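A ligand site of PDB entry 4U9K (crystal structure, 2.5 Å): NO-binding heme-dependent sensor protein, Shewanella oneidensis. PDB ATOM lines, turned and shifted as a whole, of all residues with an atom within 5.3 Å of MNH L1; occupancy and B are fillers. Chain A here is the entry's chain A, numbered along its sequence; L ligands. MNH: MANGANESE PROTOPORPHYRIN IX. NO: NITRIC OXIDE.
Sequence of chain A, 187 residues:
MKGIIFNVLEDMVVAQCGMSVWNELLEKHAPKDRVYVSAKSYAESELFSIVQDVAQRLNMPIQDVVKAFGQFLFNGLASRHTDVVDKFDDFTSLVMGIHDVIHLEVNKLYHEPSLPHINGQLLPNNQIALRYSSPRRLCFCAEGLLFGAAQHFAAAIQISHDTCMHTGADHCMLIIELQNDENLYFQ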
ATOM      1  N   MET A   1      -6.673 -16.667 -16.743  1.00  0.00           N
ATOM      2  CA  MET A   1      -7.740 -16.516 -15.722  1.00  0.00           C
ATOM      3  C   MET A   1      -8.202 -17.894 -15.266  1.00  0.00           C
ATOM      4  O   MET A   1      -8.577 -18.737 -16.097  1.00  0.00           O
ATOM      5  CB  MET A   1      -8.912 -15.706 -16.302  1.00  0.00           C
ATOM      6  CG  MET A   1      -9.961 -15.323 -15.278  1.00  0.00           C
ATOM      7  SD  MET A   1      -9.376 -13.884 -14.335  1.00  0.00           S
ATOM      8  CE  MET A   1      -9.414 -12.550 -15.560  1.00  0.00           C
ATOM      9  N   LYS A   2      -8.125 -18.133 -13.959  1.00  0.00           N
ATOM     10  CA  LYS A   2      -8.460 -19.462 -13.383  1.00  0.00           C
ATOM     11  C   LYS A   2      -9.919 -19.804 -13.474  1.00  0.00           C
ATOM     12  O   LYS A   2     -10.780 -18.949 -13.397  1.00  0.00           O
ATOM     13  CB  LYS A   2      -8.003 -19.551 -11.925  1.00  0.00           C
ATOM     14  CG  LYS A   2      -6.480 -19.542 -11.770  1.00  0.00           C
ATOM     15  CD  LYS A   2      -5.873 -20.723 -12.495  1.00  0.00           C
ATOM     16  CE  LYS A   2      -4.421 -20.814 -12.203  1.00  0.00           C
ATOM     17  NZ  LYS A   2      -3.874 -21.903 -13.027  1.00  0.00           N
ATOM     18  N   ILE A   4     -11.887 -21.057 -11.522  1.00  0.00           N
ATOM     19  CA  ILE A   4     -12.690 -20.725 -10.385  1.00  0.00           C
ATOM     20  C   ILE A   4     -13.386 -19.380 -10.590  1.00  0.00           C
ATOM     21  O   ILE A   4     -14.523 -19.197 -10.111  1.00  0.00           O
ATOM     22  CB  ILE A   4     -11.896 -20.663  -9.072  1.00  0.00           C
ATOM     23  CG1 ILE A   4     -12.836 -20.232  -7.939  1.00  0.00           C
ATOM     24  CG2 ILE A   4     -10.723 -19.689  -9.155  1.00  0.00           C
ATOM     25  CD1 ILE A   4     -12.573 -20.941  -6.771  1.00  0.00           C
ATOM     26  N   ILE A   5     -12.740 -18.460 -11.299  1.00  0.00           N
ATOM     27  CA  ILE A   5     -13.326 -17.152 -11.496  1.00  0.00           C
ATOM     28  C   ILE A   5     -14.522 -17.322 -12.435  1.00  0.00           C
ATOM     29  O   ILE A   5     -15.590 -16.735 -12.195  1.00  0.00           O
ATOM     30  CB  ILE A   5     -12.322 -16.149 -12.076  1.00  0.00           C
ATOM     31  CG1 ILE A   5     -11.081 -16.063 -11.198  1.00  0.00           C
ATOM     32  CG2 ILE A   5     -12.950 -14.803 -12.237  1.00  0.00           C
ATOM     33  CD1 ILE A   5     -11.279 -15.639  -9.796  1.00  0.00           C
ATOM     34  N   SER A  41      -5.942 -22.661 -15.870  1.00  0.00           N
ATOM     35  CA  SER A  41      -5.897 -21.340 -16.500  1.00  0.00           C
ATOM     36  C   SER A  41      -6.633 -21.355 -17.810  1.00  0.00           C
ATOM     37  O   SER A  41      -6.472 -22.288 -18.572  1.00  0.00           O
ATOM     38  CB  SER A  41      -4.472 -20.914 -16.782  1.00  0.00           C
ATOM     39  OG  SER A  41      -3.755 -20.701 -15.582  1.00  0.00           O
ATOM     40  N   PHE A  74     -16.227 -12.162  -3.976  1.00  0.00           N
ATOM     41  CA  PHE A  74     -15.596 -12.314  -2.681  1.00  0.00           C
ATOM     42  C   PHE A  74     -16.259 -13.444  -1.931  1.00  0.00           C
ATOM     43  O   PHE A  74     -15.587 -14.271  -1.357  1.00  0.00           O
ATOM     44  CB  PHE A  74     -15.674 -11.099  -1.800  1.00  0.00           C
ATOM     45  CG  PHE A  74     -14.872 -11.266  -0.548  1.00  0.00           C
ATOM     46  CD1 PHE A  74     -15.426 -11.848   0.553  1.00  0.00           C
ATOM     47  CD2 PHE A  74     -13.526 -10.916  -0.521  1.00  0.00           C
ATOM     48  CE1 PHE A  74     -14.688 -12.041   1.684  1.00  0.00           C
ATOM     49  CE2 PHE A  74     -12.769 -11.086   0.593  1.00  0.00           C
ATOM     50  CZ  PHE A  74     -13.347 -11.667   1.714  1.00  0.00           C
ATOM     51  N   LEU A  77     -15.301 -16.827  -3.453  1.00  0.00           N
ATOM     52  CA  LEU A  77     -13.950 -17.218  -3.067  1.00  0.00           C
ATOM     53  C   LEU A  77     -13.877 -17.609  -1.614  1.00  0.00           C
ATOM     54  O   LEU A  77     -13.286 -18.654  -1.320  1.00  0.00           O
ATOM     55  CB  LEU A  77     -12.928 -16.130  -3.302  1.00  0.00           C
ATOM     56  CG  LEU A  77     -12.657 -15.856  -4.782  1.00  0.00           C
ATOM     57  CD1 LEU A  77     -11.825 -14.611  -4.912  1.00  0.00           C
ATOM     58  CD2 LEU A  77     -11.981 -16.978  -5.463  1.00  0.00           C
ATOM     59  N   ALA A  78     -14.449 -16.809  -0.735  1.00  0.00           N
ATOM     60  CA  ALA A  78     -14.403 -17.087   0.708  1.00  0.00           C
ATOM     61  C   ALA A  78     -15.049 -18.413   1.030  1.00  0.00           C
ATOM     62  O   ALA A  78     -14.625 -19.094   1.967  1.00  0.00           O
ATOM     63  CB  ALA A  78     -15.086 -16.020   1.497  1.00  0.00           C
ATOM     64  N   HIS A  81     -12.463 -21.101  -0.415  1.00  0.00           N
ATOM     65  CA  HIS A  81     -11.185 -21.062   0.293  1.00  0.00           C
ATOM     66  C   HIS A  81     -11.404 -20.540   1.717  1.00  0.00           C
ATOM     67  O   HIS A  81     -10.742 -19.604   2.163  1.00  0.00           O
ATOM     68  CB  HIS A  81     -10.171 -20.156  -0.465  1.00  0.00           C
ATOM     69  CG  HIS A  81      -9.793 -20.678  -1.822  1.00  0.00           C
ATOM     70  ND1 HIS A  81      -9.139 -21.870  -2.012  1.00  0.00           N
ATOM     71  CD2 HIS A  81     -10.030 -20.196  -3.063  1.00  0.00           C
ATOM     72  CE1 HIS A  81      -8.978 -22.100  -3.303  1.00  0.00           C
ATOM     73  NE2 HIS A  81      -9.520 -21.087  -3.960  1.00  0.00           N
ATOM     74  N   VAL A  84      -8.473 -19.822   3.988  1.00  0.00           N
ATOM     75  CA  VAL A  84      -7.707 -18.609   3.774  1.00  0.00           C
ATOM     76  C   VAL A  84      -8.359 -17.361   4.452  1.00  0.00           C
ATOM     77  O   VAL A  84      -7.679 -16.610   5.176  1.00  0.00           O
ATOM     78  CB  VAL A  84      -7.516 -18.316   2.250  1.00  0.00           C
ATOM     79  CG1 VAL A  84      -6.811 -17.052   2.044  1.00  0.00           C
ATOM     80  CG2 VAL A  84      -6.740 -19.471   1.593  1.00  0.00           C
ATOM     81  N   VAL A  85      -9.659 -17.148   4.217  1.00  0.00           N
ATOM     82  CA  VAL A  85     -10.375 -15.978   4.788  1.00  0.00           C
ATOM     83  C   VAL A  85     -10.537 -16.078   6.319  1.00  0.00           C
ATOM     84  O   VAL A  85     -10.533 -15.069   6.988  1.00  0.00           O
ATOM     85  CB  VAL A  85     -11.740 -15.806   4.142  1.00  0.00           C
ATOM     86  CG1 VAL A  85     -12.534 -14.742   4.822  1.00  0.00           C
ATOM     87  CG2 VAL A  85     -11.586 -15.425   2.683  1.00  0.00           C
ATOM     88  N   LEU A  94      -7.726  -8.258   6.817  1.00  0.00           N
ATOM     89  CA  LEU A  94      -7.826  -8.951   5.555  1.00  0.00           C
ATOM     90  C   LEU A  94      -7.286  -8.051   4.414  1.00  0.00           C
ATOM     91  O   LEU A  94      -6.510  -8.501   3.582  1.00  0.00           O
ATOM     92  CB  LEU A  94      -9.257  -9.405   5.291  1.00  0.00           C
ATOM     93  CG  LEU A  94      -9.471 -10.216   4.020  1.00  0.00           C
ATOM     94  CD1 LEU A  94     -10.581 -11.203   4.123  1.00  0.00           C
ATOM     95  CD2 LEU A  94      -9.784  -9.296   2.815  1.00  0.00           C
ATOM     96  N   ILE A  98      -4.042  -9.008   1.699  1.00  0.00           N
ATOM     97  CA  ILE A  98      -4.442  -9.503   0.400  1.00  0.00           C
ATOM     98  C   ILE A  98      -3.204  -9.943  -0.340  1.00  0.00           C
ATOM     99  O   ILE A  98      -3.228 -10.975  -0.991  1.00  0.00           O
ATOM    100  CB  ILE A  98      -5.147  -8.484  -0.427  1.00  0.00           C
ATOM    101  CG1 ILE A  98      -6.470  -8.166   0.226  1.00  0.00           C
ATOM    102  CG2 ILE A  98      -5.425  -9.016  -1.846  1.00  0.00           C
ATOM    103  CD1 ILE A  98      -6.974  -6.778  -0.133  1.00  0.00           C
ATOM    104  N   ILE A 102      -3.187 -13.819   1.418  1.00  0.00           N
ATOM    105  CA  ILE A 102      -4.213 -14.403   0.560  1.00  0.00           C
ATOM    106  C   ILE A 102      -3.649 -14.772  -0.822  1.00  0.00           C
ATOM    107  O   ILE A 102      -3.612 -15.930  -1.182  1.00  0.00           O
ATOM    108  CB  ILE A 102      -5.398 -13.421   0.405  1.00  0.00           C
ATOM    109  CG1 ILE A 102      -6.034 -13.155   1.754  1.00  0.00           C
ATOM    110  CG2 ILE A 102      -6.454 -14.004  -0.522  1.00  0.00           C
ATOM    111  CD1 ILE A 102      -7.225 -12.281   1.671  1.00  0.00           C
ATOM    112  N   HIS A 103      -3.221 -13.795  -1.604  1.00  0.00           N
ATOM    113  CA  HIS A 103      -2.746 -14.103  -2.938  1.00  0.00           C
ATOM    114  C   HIS A 103      -1.359 -14.848  -2.819  1.00  0.00           C
ATOM    115  O   HIS A 103      -0.949 -15.587  -3.734  1.00  0.00           O
ATOM    116  CB  HIS A 103      -2.669 -12.828  -3.779  1.00  0.00           C
ATOM    117  CG  HIS A 103      -3.998 -12.267  -4.217  1.00  0.00           C
ATOM    118  ND1 HIS A 103      -4.154 -11.001  -4.709  1.00  0.00           N
ATOM    119  CD2 HIS A 103      -5.259 -12.817  -4.236  1.00  0.00           C
ATOM    120  CE1 HIS A 103      -5.421 -10.794  -5.030  1.00  0.00           C
ATOM    121  NE2 HIS A 103      -6.123 -11.855  -4.725  1.00  0.00           N
ATOM    122  N   VAL A 106      -2.643 -18.280  -2.746  1.00  0.00           N
ATOM    123  CA  VAL A 106      -3.176 -18.558  -4.078  1.00  0.00           C
ATOM    124  C   VAL A 106      -2.019 -19.057  -4.966  1.00  0.00           C
ATOM    125  O   VAL A 106      -2.230 -20.006  -5.736  1.00  0.00           O
ATOM    126  CB  VAL A 106      -3.905 -17.324  -4.693  1.00  0.00           C
ATOM    127  CG1 VAL A 106      -4.387 -17.577  -6.107  1.00  0.00           C
ATOM    128  CG2 VAL A 106      -5.093 -16.989  -3.894  1.00  0.00           C
ATOM    129  N   TYR A 110      -2.767 -22.847  -6.542  1.00  0.00           N
ATOM    130  CA  TYR A 110      -2.974 -22.828  -7.977  1.00  0.00           C
ATOM    131  C   TYR A 110      -1.616 -22.809  -8.716  1.00  0.00           C
ATOM    132  O   TYR A 110      -0.681 -22.108  -8.313  1.00  0.00           O
ATOM    133  CB  TYR A 110      -3.773 -21.588  -8.408  1.00  0.00           C
ATOM    134  CG  TYR A 110      -5.190 -21.564  -7.915  1.00  0.00           C
ATOM    135  CD1 TYR A 110      -5.513 -20.968  -6.736  1.00  0.00           C
ATOM    136  CD2 TYR A 110      -6.200 -22.194  -8.617  1.00  0.00           C
ATOM    137  CE1 TYR A 110      -6.808 -20.979  -6.263  1.00  0.00           C
ATOM    138  CE2 TYR A 110      -7.505 -22.217  -8.160  1.00  0.00           C
ATOM    139  CZ  TYR A 110      -7.789 -21.612  -6.970  1.00  0.00           C
ATOM    140  OH  TYR A 110      -9.076 -21.616  -6.469  1.00  0.00           O
ATOM    141  N   GLU A 112       0.811 -21.314 -11.173  1.00  0.00           N
ATOM    142  CA  GLU A 112       1.042 -20.037 -11.914  1.00  0.00           C
ATOM    143  C   GLU A 112      -0.215 -19.174 -12.159  1.00  0.00           C
ATOM    144  O   GLU A 112      -0.602 -18.901 -13.324  1.00  0.00           O
ATOM    145  CB  GLU A 112       1.743 -20.362 -13.266  1.00  0.00           C
ATOM    146  CG  GLU A 112       3.138 -20.996 -13.047  1.00  0.00           C
ATOM    147  CD  GLU A 112       3.823 -21.352 -14.330  1.00  0.00           C
ATOM    148  OE1 GLU A 112       3.285 -20.986 -15.385  1.00  0.00           O
ATOM    149  OE2 GLU A 112       4.899 -22.024 -14.323  1.00  0.00           O
ATOM    150  N   PRO A 113      -0.868 -18.722 -11.063  1.00  0.00           N
ATOM    151  CA  PRO A 113      -1.993 -17.798 -11.213  1.00  0.00           C
ATOM    152  C   PRO A 113      -1.547 -16.430 -11.701  1.00  0.00           C
ATOM    153  O   PRO A 113      -0.368 -16.103 -11.546  1.00  0.00           O
ATOM    154  CB  PRO A 113      -2.563 -17.679  -9.784  1.00  0.00           C
ATOM    155  CG  PRO A 113      -1.340 -17.768  -8.934  1.00  0.00           C
ATOM    156  CD  PRO A 113      -0.485 -18.869  -9.639  1.00  0.00           C
ATOM    157  N   SER A 114      -2.497 -15.650 -12.251  1.00  0.00           N
ATOM    158  CA  SER A 114      -2.264 -14.278 -12.757  1.00  0.00           C
ATOM    159  C   SER A 114      -2.939 -13.263 -11.840  1.00  0.00           C
ATOM    160  O   SER A 114      -4.169 -13.040 -11.896  1.00  0.00           O
ATOM    161  CB  SER A 114      -2.770 -14.135 -14.188  1.00  0.00           C
ATOM    162  OG  SER A 114      -1.921 -14.821 -15.121  1.00  0.00           O
ATOM    163  N   LEU A 115      -2.124 -12.689 -10.984  1.00  0.00           N
ATOM    164  CA  LEU A 115      -2.582 -11.914  -9.864  1.00  0.00           C
ATOM    165  C   LEU A 115      -2.112 -10.462  -9.942  1.00  0.00           C
ATOM    166  O   LEU A 115      -1.069 -10.167 -10.527  1.00  0.00           O
ATOM    167  CB  LEU A 115      -2.098 -12.531  -8.562  1.00  0.00           C
ATOM    168  CG  LEU A 115      -2.703 -13.880  -8.268  1.00  0.00           C
ATOM    169  CD1 LEU A 115      -1.810 -14.583  -7.214  1.00  0.00           C
ATOM    170  CD2 LEU A 115      -4.162 -13.692  -7.795  1.00  0.00           C
ATOM    171  N   PRO A 116      -2.890  -9.547  -9.336  1.00  0.00           N
ATOM    172  CA  PRO A 116      -2.419  -8.162  -9.384  1.00  0.00           C
ATOM    173  C   PRO A 116      -1.314  -7.974  -8.387  1.00  0.00           C
ATOM    174  O   PRO A 116      -1.023  -8.883  -7.591  1.00  0.00           O
ATOM    175  CB  PRO A 116      -3.655  -7.373  -9.036  1.00  0.00           C
ATOM    176  CG  PRO A 116      -4.291  -8.250  -7.940  1.00  0.00           C
ATOM    177  CD  PRO A 116      -4.079  -9.681  -8.483  1.00  0.00           C
ATOM    178  N   ILE A 118      -0.530  -5.656  -5.175  1.00  0.00           N
ATOM    179  CA  ILE A 118      -1.295  -4.886  -4.232  1.00  0.00           C
ATOM    180  C   ILE A 118      -0.413  -4.529  -3.057  1.00  0.00           C
ATOM    181  O   ILE A 118       0.372  -5.346  -2.644  1.00  0.00           O
ATOM    182  CB  ILE A 118      -2.530  -5.650  -3.777  1.00  0.00           C
ATOM    183  CG1 ILE A 118      -3.502  -5.715  -4.961  1.00  0.00           C
ATOM    184  CG2 ILE A 118      -3.202  -4.950  -2.596  1.00  0.00           C
ATOM    185  CD1 ILE A 118      -4.705  -6.405  -4.712  1.00  0.00           C
ATOM    186  N   LEU A 130      -4.882   1.518  -0.520  1.00  0.00           N
ATOM    187  CA  LEU A 130      -4.611   0.280  -1.219  1.00  0.00           C
ATOM    188  C   LEU A 130      -4.144   0.540  -2.664  1.00  0.00           C
ATOM    189  O   LEU A 130      -4.937   0.907  -3.520  1.00  0.00           O
ATOM    190  CB  LEU A 130      -5.849  -0.578  -1.256  1.00  0.00           C
ATOM    191  CG  LEU A 130      -5.559  -2.035  -1.510  1.00  0.00           C
ATOM    192  CD1 LEU A 130      -4.835  -2.662  -0.292  1.00  0.00           C
ATOM    193  CD2 LEU A 130      -6.845  -2.800  -1.797  1.00  0.00           C
ATOM    194  N   TYR A 132      -3.117  -0.559  -6.261  1.00  0.00           N
ATOM    195  CA  TYR A 132      -3.313  -1.718  -7.128  1.00  0.00           C
ATOM    196  C   TYR A 132      -2.606  -1.506  -8.427  1.00  0.00           C
ATOM    197  O   TYR A 132      -2.471  -0.406  -8.906  1.00  0.00           O
ATOM    198  CB  TYR A 132      -4.796  -1.966  -7.368  1.00  0.00           C
ATOM    199  CG  TYR A 132      -5.172  -2.861  -8.492  1.00  0.00           C
ATOM    200  CD1 TYR A 132      -5.242  -2.406  -9.775  1.00  0.00           C
ATOM    201  CD2 TYR A 132      -5.540  -4.142  -8.268  1.00  0.00           C
ATOM    202  CE1 TYR A 132      -5.619  -3.253 -10.826  1.00  0.00           C
ATOM    203  CE2 TYR A 132      -5.937  -4.989  -9.307  1.00  0.00           C
ATOM    204  CZ  TYR A 132      -5.961  -4.528 -10.587  1.00  0.00           C
ATOM    205  OH  TYR A 132      -6.354  -5.347 -11.618  1.00  0.00           O
ATOM    206  N   SER A 134      -1.945  -3.911 -12.185  1.00  0.00           N
ATOM    207  CA  SER A 134      -2.053  -5.149 -12.949  1.00  0.00           C
ATOM    208  C   SER A 134      -2.246  -4.806 -14.383  1.00  0.00           C
ATOM    209  O   SER A 134      -2.965  -3.852 -14.690  1.00  0.00           O
ATOM    210  CB  SER A 134      -3.207  -6.001 -12.517  1.00  0.00           C
ATOM    211  OG  SER A 134      -3.630  -6.818 -13.593  1.00  0.00           O
ATOM    212  N   PRO A 135      -1.644  -5.587 -15.272  1.00  0.00           N
ATOM    213  CA  PRO A 135      -1.831  -5.350 -16.688  1.00  0.00           C
ATOM    214  C   PRO A 135      -3.270  -5.685 -17.085  1.00  0.00           C
ATOM    215  O   PRO A 135      -3.719  -5.327 -18.153  1.00  0.00           O
ATOM    216  CB  PRO A 135      -0.804  -6.322 -17.335  1.00  0.00           C
ATOM    217  CG  PRO A 135      -0.737  -7.426 -16.381  1.00  0.00           C
ATOM    218  CD  PRO A 135      -0.812  -6.783 -15.039  1.00  0.00           C
ATOM    219  N   ARG A 136      -3.981  -6.423 -16.269  1.00  0.00           N
ATOM    220  CA  ARG A 136      -5.366  -6.707 -16.606  1.00  0.00           C
ATOM    221  C   ARG A 136      -6.332  -5.533 -16.286  1.00  0.00           C
ATOM    222  O   ARG A 136      -7.468  -5.517 -16.755  1.00  0.00           O
ATOM    223  CB  ARG A 136      -5.824  -7.968 -15.896  1.00  0.00           C
ATOM    224  CG  ARG A 136      -5.254  -9.226 -16.602  1.00  0.00           C
ATOM    225  CD  ARG A 136      -5.262 -10.424 -15.637  1.00  0.00           C
ATOM    226  NE  ARG A 136      -4.274 -10.292 -14.544  1.00  0.00           N
ATOM    227  CZ  ARG A 136      -2.974 -10.484 -14.693  1.00  0.00           C
ATOM    228  NH1 ARG A 136      -2.477 -10.803 -15.876  1.00  0.00           N
ATOM    229  NH2 ARG A 136      -2.153 -10.341 -13.664  1.00  0.00           N
ATOM    230  N   LEU A 138      -8.048  -4.514 -13.598  1.00  0.00           N
ATOM    231  CA  LEU A 138      -9.324  -4.901 -12.995  1.00  0.00           C
ATOM    232  C   LEU A 138      -9.531  -4.252 -11.655  1.00  0.00           C
ATOM    233  O   LEU A 138     -10.030  -4.887 -10.725  1.00  0.00           O
ATOM    234  CB  LEU A 138      -9.409  -6.423 -12.855  1.00  0.00           C
ATOM    235  CG  LEU A 138      -9.526  -7.128 -14.223  1.00  0.00           C
ATOM    236  CD1 LEU A 138      -9.227  -8.652 -14.050  1.00  0.00           C
ATOM    237  CD2 LEU A 138     -10.947  -6.926 -14.717  1.00  0.00           C
ATOM    238  N   CYS A 141     -12.979  -4.560 -10.323  1.00  0.00           N
ATOM    239  CA  CYS A 141     -13.219  -5.861  -9.741  1.00  0.00           C
ATOM    240  C   CYS A 141     -12.681  -5.821  -8.323  1.00  0.00           C
ATOM    241  O   CYS A 141     -13.278  -6.349  -7.410  1.00  0.00           O
ATOM    242  CB  CYS A 141     -12.540  -6.994 -10.516  1.00  0.00           C
ATOM    243  SG  CYS A 141     -13.159  -8.584  -9.940  1.00  0.00           S
ATOM    244  N   ALA A 142     -11.560  -5.145  -8.134  1.00  0.00           N
ATOM    245  CA  ALA A 142     -10.992  -5.034  -6.787  1.00  0.00           C
ATOM    246  C   ALA A 142     -11.874  -4.232  -5.830  1.00  0.00           C
ATOM    247  O   ALA A 142     -11.943  -4.574  -4.642  1.00  0.00           O
ATOM    248  CB  ALA A 142      -9.645  -4.426  -6.835  1.00  0.00           C
ATOM    249  N   LEU A 145     -14.561  -6.547  -4.745  1.00  0.00           N
ATOM    250  CA  LEU A 145     -14.055  -7.523  -3.754  1.00  0.00           C
ATOM    251  C   LEU A 145     -13.930  -6.888  -2.364  1.00  0.00           C
ATOM    252  O   LEU A 145     -14.176  -7.548  -1.371  1.00  0.00           O
ATOM    253  CB  LEU A 145     -12.694  -8.109  -4.169  1.00  0.00           C
ATOM    254  CG  LEU A 145     -12.887  -9.038  -5.360  1.00  0.00           C
ATOM    255  CD1 LEU A 145     -11.642  -9.044  -6.251  1.00  0.00           C
ATOM    256  CD2 LEU A 145     -13.188 -10.410  -4.898  1.00  0.00           C
ATOM    257  N   LEU A 146     -13.559  -5.601  -2.319  1.00  0.00           N
ATOM    258  CA  LEU A 146     -13.404  -4.926  -1.041  1.00  0.00           C
ATOM    259  C   LEU A 146     -14.759  -4.740  -0.413  1.00  0.00           C
ATOM    260  O   LEU A 146     -14.890  -4.889   0.784  1.00  0.00           O
ATOM    261  CB  LEU A 146     -12.682  -3.613  -1.163  1.00  0.00           C
ATOM    262  CG  LEU A 146     -11.220  -3.829  -1.530  1.00  0.00           C
ATOM    263  CD1 LEU A 146     -10.669  -2.581  -2.053  1.00  0.00           C
ATOM    264  CD2 LEU A 146     -10.401  -4.265  -0.358  1.00  0.00           C
ATOM    265  N   ALA A 149     -15.656  -8.143   0.982  1.00  0.00           N
ATOM    266  CA  ALA A 149     -14.920  -8.340   2.199  1.00  0.00           C
ATOM    267  C   ALA A 149     -15.572  -7.565   3.349  1.00  0.00           C
ATOM    268  O   ALA A 149     -15.785  -8.093   4.441  1.00  0.00           O
ATOM    269  CB  ALA A 149     -13.438  -7.945   1.998  1.00  0.00           C
HETATM  270 MN   MNH L   1      -8.165 -12.113  -5.477  1.00  0.00          MN
HETATM  271  CHA MNH L   1      -7.585 -12.508  -8.529  1.00  0.00           C
HETATM  272  CHB MNH L   1      -8.044  -8.853  -5.830  1.00  0.00           C
HETATM  273  CHC MNH L   1      -9.361 -11.701  -2.368  1.00  0.00           C
HETATM  274  CHD MNH L   1      -7.934 -15.256  -4.921  1.00  0.00           C
HETATM  275  NA  MNH L   1      -7.555 -10.806  -7.015  1.00  0.00           N
HETATM  276  C1A MNH L   1      -7.658 -11.148  -8.354  1.00  0.00           C
HETATM  277  C2A MNH L   1      -7.877  -9.990  -9.226  1.00  0.00           C
HETATM  278  C3A MNH L   1      -8.057  -8.915  -8.426  1.00  0.00           C
HETATM  279  C4A MNH L   1      -7.896  -9.443  -7.077  1.00  0.00           C
HETATM  280  CMA MNH L   1      -8.382  -7.466  -8.683  1.00  0.00           C
HETATM  281  CAA MNH L   1      -7.972 -10.072 -10.783  1.00  0.00           C
HETATM  282  CBA MNH L   1      -6.631 -10.084 -11.500  1.00  0.00           C
HETATM  283  CGA MNH L   1      -5.720  -8.895 -11.589  1.00  0.00           C
HETATM  284  O1A MNH L   1      -4.593  -9.016 -12.150  1.00  0.00           O
HETATM  285  O2A MNH L   1      -6.238  -7.861 -11.087  1.00  0.00           O
HETATM  286  NB  MNH L   1      -8.461 -10.365  -4.164  1.00  0.00           N
HETATM  287  C1B MNH L   1      -8.489  -9.027  -4.515  1.00  0.00           C
HETATM  288  C2B MNH L   1      -8.874  -8.092  -3.461  1.00  0.00           C
HETATM  289  C3B MNH L   1      -9.242  -9.057  -2.558  1.00  0.00           C
HETATM  290  C4B MNH L   1      -9.069 -10.425  -2.922  1.00  0.00           C
HETATM  291  CMB MNH L   1      -8.867  -6.566  -3.580  1.00  0.00           C
HETATM  292  CAB MNH L   1      -9.806  -8.778  -1.189  1.00  0.00           C
HETATM  293  CBB MNH L   1     -11.080  -8.298  -0.581  1.00  0.00           C
HETATM  294  NC  MNH L   1      -8.596 -13.380  -3.758  1.00  0.00           N
HETATM  295  C1C MNH L   1      -9.234 -13.065  -2.569  1.00  0.00           C
HETATM  296  C2C MNH L   1      -9.544 -14.270  -1.813  1.00  0.00           C
HETATM  297  C3C MNH L   1      -9.117 -15.264  -2.592  1.00  0.00           C
HETATM  298  C4C MNH L   1      -8.504 -14.756  -3.770  1.00  0.00           C
HETATM  299  CMC MNH L   1     -10.232 -14.300  -0.448  1.00  0.00           C
HETATM  300  CAC MNH L   1      -9.144 -16.743  -2.339  1.00  0.00           C
HETATM  301  CBC MNH L   1      -8.180 -17.361  -1.406  1.00  0.00           C
HETATM  302  ND  MNH L   1      -7.593 -13.771  -6.607  1.00  0.00           N
HETATM  303  C1D MNH L   1      -7.686 -15.121  -6.283  1.00  0.00           C
HETATM  304  C2D MNH L   1      -7.559 -15.971  -7.466  1.00  0.00           C
HETATM  305  C3D MNH L   1      -7.348 -15.090  -8.464  1.00  0.00           C
HETATM  306  C4D MNH L   1      -7.480 -13.762  -7.976  1.00  0.00           C
HETATM  307  CMD MNH L   1      -7.591 -17.479  -7.527  1.00  0.00           C
HETATM  308  CAD MNH L   1      -7.256 -15.428  -9.944  1.00  0.00           C
HETATM  309  CBD MNH L   1      -5.870 -15.489 -10.534  1.00  0.00           C
HETATM  310  CGD MNH L   1      -5.973 -16.080 -11.945  1.00  0.00           C
HETATM  311  O1D MNH L   1      -7.101 -16.091 -12.500  1.00  0.00           O
HETATM  312  O2D MNH L   1      -4.950 -16.615 -12.521  1.00  0.00           O
HETATM  313  N    NO L   2      -9.614 -12.187  -6.055  1.00  0.00           N
HETATM  314  O    NO L   2     -10.676 -12.215  -6.953  1.00  0.00           O
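MN of MNH L1 is bound by NE2 of His 103, at 2.2 Å.
The side-chain hydroxyl (OH) of Tyr 132 lies within hydrogen-bond range of an oxygen (O2A) of MNH L1.
The backbone NH of Ser 114 lies within hydrogen-bond range of an oxygen (O2D) of MNH L1.
An oxygen (O1D) of MNH L1 sits at hydrogen-bond distance from the backbone NH of Lys 2 (2.7 Å).
NE of Arg 136 lies within salt-bridge range of O1A of MNH L1, at 2.7 Å.
An oxygen (O1A) of MNH L1 lies within hydrogen-bond range of the side-chain hydroxyl of Ser 134.
A nitrogen (N) of NO L2 binds a manganese atom (MN) of MNH L1 (1.6 Å).
The backbone carbonyl oxygen (O) of Ile 98 sits at hydrogen-bond distance from the backbone NH (N) of His 103 (2.9 Å).
The side-chain hydroxyl of Tyr 132 is in hydrogen-bond range of the backbone NH of Leu 138 (2.7 Å).
The side-chain amino group (NZ) of Lys 2 sits at hydrogen-bond distance from the side-chain hydroxyl (OG) of Ser 41 (2.8 Å).
The side-chain hydroxyl (OG) of Ser 134 sits at hydrogen-bond distance from the backbone NH (N) of Arg 136 (2.7 Å).
The guanidinium group (NH2) of Arg 136 sits at hydrogen-bond distance from the backbone carbonyl oxygen (O) of Leu 115.
NE2 of His 81 sits at hydrogen-bond distance from OH of Tyr 110 (2.6 Å).
SD of Met 1 sits close to O1D of MNH L1 (3.7 Å).
The backbone nitrogen (N) of Pro 116 lies close to an oxygen (O1A) of MNH L1.
Residues that only touch MNH L1: Leu 145 (3.3 Å), Leu 115 (3.3 Å), Ile 102 (3.4 Å), Pro 113 (3.4 Å), Phe 74 (3.5 Å), Val 106 (3.5 Å), Ala 149 (3.5 Å), Leu 77 (3.5 Å), His 81 (3.6 Å), Val 85 (3.6 Å), Ile 98 (3.6 Å), Leu 138 (3.7 Å), Val 84 (3.7 Å), Leu 94 (3.8 Å), Ala 142 (3.8 Å) and Tyr 110 (3.8 Å).
Hydrophobic or aromatic side chains that line MNH L1: Met 1, Phe 74, Leu 77, His 81, Val 84, Val 85, Leu 94, Ile 98, Ile 102, His 103, Val 106, Tyr 110, Pro 113, Leu 115, Pro 116, Tyr 132, Leu 138, Ala 142, Leu 145 and Ala 149.
Of the 34 residues printed, 24 come within 4 Å of MNH L1.
Along chain A the residues within 4 Å of MNH L1 span positions 1 to 149.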
